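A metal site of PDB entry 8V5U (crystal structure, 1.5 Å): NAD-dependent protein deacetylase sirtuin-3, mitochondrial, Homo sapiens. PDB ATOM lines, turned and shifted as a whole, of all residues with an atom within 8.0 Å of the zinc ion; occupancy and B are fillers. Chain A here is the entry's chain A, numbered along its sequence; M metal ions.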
ATOM      1  N   THR A 138      30.692  23.564   0.040  1.00  0.00           N
ATOM      2  CA  THR A 138      29.581  24.457  -0.150  1.00  0.00           C
ATOM      3  C   THR A 138      28.874  24.573   1.190  1.00  0.00           C
ATOM      4  O   THR A 138      28.544  23.567   1.808  1.00  0.00           O
ATOM      5  CB  THR A 138      28.634  23.924  -1.225  1.00  0.00           C
ATOM      6  OG1 THR A 138      29.385  23.823  -2.429  1.00  0.00           O
ATOM      7  CG2 THR A 138      27.458  24.856  -1.467  1.00  0.00           C
ATOM      8  N   CYS A 139      28.500  25.808   1.566  1.00  0.00           N
ATOM      9  CA  CYS A 139      27.673  25.948   2.749  1.00  0.00           C
ATOM     10  C   CYS A 139      26.287  25.373   2.507  1.00  0.00           C
ATOM     11  O   CYS A 139      25.660  25.639   1.484  1.00  0.00           O
ATOM     12  CB  CYS A 139      27.611  27.432   3.081  1.00  0.00           C
ATOM     13  SG  CYS A 139      26.590  27.725   4.549  1.00  0.00           S
ATOM     14  N   THR A 140      25.797  24.592   3.476  1.00  0.00           N
ATOM     15  CA  THR A 140      24.524  23.906   3.368  1.00  0.00           C
ATOM     16  C   THR A 140      23.341  24.877   3.495  1.00  0.00           C
ATOM     17  O   THR A 140      22.210  24.474   3.188  1.00  0.00           O
ATOM     18  CB  THR A 140      24.494  22.817   4.430  1.00  0.00           C
ATOM     19  OG1 THR A 140      24.692  23.434   5.712  1.00  0.00           O
ATOM     20  CG2 THR A 140      25.541  21.753   4.145  1.00  0.00           C
ATOM     21  N   VAL A 141      23.594  26.096   3.977  1.00  0.00           N
ATOM     22  CA  VAL A 141      22.497  27.045   4.168  1.00  0.00           C
ATOM     23  C   VAL A 141      22.542  28.134   3.104  1.00  0.00           C
ATOM     24  O   VAL A 141      21.589  28.255   2.339  1.00  0.00           O
ATOM     25  CB  VAL A 141      22.553  27.586   5.601  1.00  0.00           C
ATOM     26  CG1 VAL A 141      21.567  28.750   5.785  1.00  0.00           C
ATOM     27  CG2 VAL A 141      22.287  26.468   6.595  1.00  0.00           C
ATOM     28  N   CYS A 142      23.656  28.880   2.983  1.00  0.00           N
ATOM     29  CA  CYS A 142      23.644  30.004   2.060  1.00  0.00           C
ATOM     30  C   CYS A 142      24.217  29.641   0.696  1.00  0.00           C
ATOM     31  O   CYS A 142      24.150  30.461  -0.207  1.00  0.00           O
ATOM     32  CB  CYS A 142      24.385  31.195   2.624  1.00  0.00           C
ATOM     33  SG  CYS A 142      26.173  30.961   2.638  1.00  0.00           S
ATOM     34  N   GLN A 143      24.815  28.444   0.545  1.00  0.00           N
ATOM     35  CA  GLN A 143      25.247  27.909  -0.755  1.00  0.00           C
ATOM     36  C   GLN A 143      26.575  28.522  -1.218  1.00  0.00           C
ATOM     37  O   GLN A 143      27.022  28.292  -2.329  1.00  0.00           O
ATOM     38  CB  GLN A 143      24.132  27.996  -1.814  1.00  0.00           C
ATOM     39  CG  GLN A 143      22.788  27.423  -1.403  1.00  0.00           C
ATOM     40  CD  GLN A 143      22.846  26.026  -0.848  1.00  0.00           C
ATOM     41  OE1 GLN A 143      23.587  25.177  -1.349  1.00  0.00           O
ATOM     42  NE2 GLN A 143      22.110  25.770   0.228  1.00  0.00           N
ATOM     43  N   ARG A 144      27.276  29.229  -0.336  1.00  0.00           N
ATOM     44  CA  ARG A 144      28.545  29.851  -0.643  1.00  0.00           C
ATOM     45  C   ARG A 144      29.586  28.766  -0.928  1.00  0.00           C
ATOM     46  O   ARG A 144      29.678  27.804  -0.163  1.00  0.00           O
ATOM     47  CB  ARG A 144      29.001  30.789   0.483  1.00  0.00           C
ATOM     48  CG  ARG A 144      30.350  31.442   0.266  1.00  0.00           C
ATOM     49  CD  ARG A 144      30.735  32.486   1.303  1.00  0.00           C
ATOM     50  NE  ARG A 144      32.098  32.961   1.022  1.00  0.00           N
ATOM     51  CZ  ARG A 144      32.378  34.106   0.399  1.00  0.00           C
ATOM     52  NH1 ARG A 144      31.394  34.899  -0.017  1.00  0.00           N
ATOM     53  NH2 ARG A 144      33.636  34.436   0.194  1.00  0.00           N
ATOM     54  N   PRO A 145      30.322  28.862  -2.061  1.00  0.00           N
ATOM     55  CA  PRO A 145      31.388  27.908  -2.386  1.00  0.00           C
ATOM     56  C   PRO A 145      32.702  28.235  -1.714  1.00  0.00           C
ATOM     57  O   PRO A 145      33.020  29.405  -1.479  1.00  0.00           O
ATOM     58  CB  PRO A 145      31.501  27.976  -3.920  1.00  0.00           C
ATOM     59  CG  PRO A 145      31.033  29.380  -4.258  1.00  0.00           C
ATOM     60  CD  PRO A 145      30.071  29.821  -3.146  1.00  0.00           C
ATOM     61  N   PHE A 146      33.454  27.180  -1.367  1.00  0.00           N
ATOM     62  CA  PHE A 146      34.696  27.319  -0.647  1.00  0.00           C
ATOM     63  C   PHE A 146      35.704  26.349  -1.226  1.00  0.00           C
ATOM     64  O   PHE A 146      35.368  25.198  -1.484  1.00  0.00           O
ATOM     65  CB  PHE A 146      34.662  26.990   0.845  1.00  0.00           C
ATOM     66  CG  PHE A 146      33.721  27.880   1.652  1.00  0.00           C
ATOM     67  CD1 PHE A 146      32.375  27.574   1.727  1.00  0.00           C
ATOM     68  CD2 PHE A 146      34.183  29.009   2.300  1.00  0.00           C
ATOM     69  CE1 PHE A 146      31.513  28.377   2.447  1.00  0.00           C
ATOM     70  CE2 PHE A 146      33.312  29.797   3.062  1.00  0.00           C
ATOM     71  CZ  PHE A 146      31.984  29.481   3.107  1.00  0.00           C
ATOM     72  N   ARG A 162      32.149  25.786  10.041  1.00  0.00           N
ATOM     73  CA  ARG A 162      31.005  26.672  10.050  1.00  0.00           C
ATOM     74  C   ARG A 162      31.223  27.783   9.015  1.00  0.00           C
ATOM     75  O   ARG A 162      32.321  28.299   8.853  1.00  0.00           O
ATOM     76  CB  ARG A 162      30.789  27.270  11.442  1.00  0.00           C
ATOM     77  CG  ARG A 162      30.506  26.292  12.578  1.00  0.00           C
ATOM     78  CD  ARG A 162      29.373  25.323  12.282  1.00  0.00           C
ATOM     79  NE  ARG A 162      28.047  25.938  12.393  1.00  0.00           N
ATOM     80  CZ  ARG A 162      27.432  26.208  13.541  1.00  0.00           C
ATOM     81  NH1 ARG A 162      27.978  25.852  14.695  1.00  0.00           N
ATOM     82  NH2 ARG A 162      26.270  26.815  13.529  1.00  0.00           N
ATOM     83  N   CYS A 163      30.136  28.174   8.357  1.00  0.00           N
ATOM     84  CA  CYS A 163      30.155  29.254   7.376  1.00  0.00           C
ATOM     85  C   CYS A 163      30.363  30.591   8.065  1.00  0.00           C
ATOM     86  O   CYS A 163      29.656  30.912   9.009  1.00  0.00           O
ATOM     87  CB  CYS A 163      28.856  29.254   6.592  1.00  0.00           C
ATOM     88  SG  CYS A 163      28.786  30.521   5.296  1.00  0.00           S
ATOM     89  N   PRO A 164      31.284  31.448   7.570  1.00  0.00           N
ATOM     90  CA  PRO A 164      31.452  32.779   8.156  1.00  0.00           C
ATOM     91  C   PRO A 164      30.290  33.729   7.865  1.00  0.00           C
ATOM     92  O   PRO A 164      30.247  34.808   8.443  1.00  0.00           O
ATOM     93  CB  PRO A 164      32.741  33.243   7.487  1.00  0.00           C
ATOM     94  CG  PRO A 164      32.702  32.584   6.147  1.00  0.00           C
ATOM     95  CD  PRO A 164      32.188  31.191   6.448  1.00  0.00           C
ATOM     96  N   VAL A 165      29.368  33.331   6.979  1.00  0.00           N
ATOM     97  CA  VAL A 165      28.308  34.220   6.561  1.00  0.00           C
ATOM     98  C   VAL A 165      27.075  33.909   7.398  1.00  0.00           C
ATOM     99  O   VAL A 165      26.477  34.824   7.986  1.00  0.00           O
ATOM    100  CB  VAL A 165      27.985  34.212   5.059  1.00  0.00           C
ATOM    101  CG1 VAL A 165      26.851  35.185   4.704  1.00  0.00           C
ATOM    102  CG2 VAL A 165      29.226  34.511   4.225  1.00  0.00           C
ATOM    103  N   CYS A 166      26.705  32.635   7.457  1.00  0.00           N
ATOM    104  CA  CYS A 166      25.415  32.257   8.035  1.00  0.00           C
ATOM    105  C   CYS A 166      25.523  31.200   9.128  1.00  0.00           C
ATOM    106  O   CYS A 166      24.496  30.758   9.618  1.00  0.00           O
ATOM    107  CB  CYS A 166      24.436  31.743   6.995  1.00  0.00           C
ATOM    108  SG  CYS A 166      25.030  30.175   6.305  1.00  0.00           S
ATOM    109  N   THR A 167      26.749  30.734   9.432  1.00  0.00           N
ATOM    110  CA  THR A 167      27.054  29.673  10.390  1.00  0.00           C
ATOM    111  C   THR A 167      26.450  28.310  10.011  1.00  0.00           C
ATOM    112  O   THR A 167      26.504  27.384  10.825  1.00  0.00           O
ATOM    113  CB  THR A 167      26.637  30.068  11.813  1.00  0.00           C
ATOM    114  OG1 THR A 167      25.217  29.948  11.812  1.00  0.00           O
ATOM    115  CG2 THR A 167      27.163  31.423  12.245  1.00  0.00           C
ATOM    116  N   GLY A 168      25.843  28.188   8.825  1.00  0.00           N
ATOM    117  CA  GLY A 168      25.557  26.869   8.266  1.00  0.00           C
ATOM    118  C   GLY A 168      26.816  25.997   8.277  1.00  0.00           C
ATOM    119  O   GLY A 168      27.939  26.460   8.357  1.00  0.00           O
ATOM    120  N   VAL A 169      26.605  24.679   8.224  1.00  0.00           N
ATOM    121  CA  VAL A 169      27.726  23.769   8.134  1.00  0.00           C
ATOM    122  C   VAL A 169      28.259  23.782   6.697  1.00  0.00           C
ATOM    123  O   VAL A 169      27.488  23.770   5.738  1.00  0.00           O
ATOM    124  CB  VAL A 169      27.277  22.373   8.622  1.00  0.00           C
ATOM    125  CG1 VAL A 169      28.277  21.275   8.286  1.00  0.00           C
ATOM    126  CG2 VAL A 169      27.008  22.372  10.119  1.00  0.00           C
ATOM    127  N   VAL A 170      29.585  23.839   6.544  1.00  0.00           N
ATOM    128  CA  VAL A 170      30.226  23.821   5.225  1.00  0.00           C
ATOM    129  C   VAL A 170      30.597  22.388   4.870  1.00  0.00           C
ATOM    130  O   VAL A 170      31.547  21.871   5.465  1.00  0.00           O
ATOM    131  CB  VAL A 170      31.480  24.705   5.134  1.00  0.00           C
ATOM    132  CG1 VAL A 170      32.126  24.582   3.754  1.00  0.00           C
ATOM    133  CG2 VAL A 170      31.219  26.167   5.469  1.00  0.00           C
HETATM  134 ZN    ZN M   1      26.634  30.027   4.642  1.00  0.00          ZN
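The backbone NH (N) of Arg 144 lies close to the side-chain sulfur (SG) of Cys 142 (3.6 Å).
The side-chain sulfur (SG) of Cys 163 sits close to the backbone NH (N) of Val 165.
The backbone NH of Cys 163 sits at hydrogen-bond distance from the backbone carbonyl oxygen of Gly 168 (2.8 Å).
The side-chain sulfur (SG) of Cys 139 lies close to the backbone NH (N) of Val 141, 3.5 Å away.
The backbone carbonyl oxygen (O) of Arg 144 sits at hydrogen-bond distance from the backbone NH (N) of Cys 139 (2.9 Å).
The backbone NH (N) of Gly 168 lies close to the side-chain sulfur (SG) of Cys 166.
Four residues have an atom within 4 Å of the zinc ion: Cys 139, Cys 142, Cys 163 and Cys 166.
The nearest printed residue that does not touch the zinc ion is Val 165 (4.4 Å).
SG of Cys 142 is bound to the zinc ion, at 2.3 Å.
SG of Cys 163 binds the zinc ion.
The zinc ion is bound by SG of Cys 139 (2.3 Å).
The zinc ion is bound by the side-chain sulfur (SG) of Cys 166 (2.3 Å).
The zinc ion has four donor atoms within binding distance.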
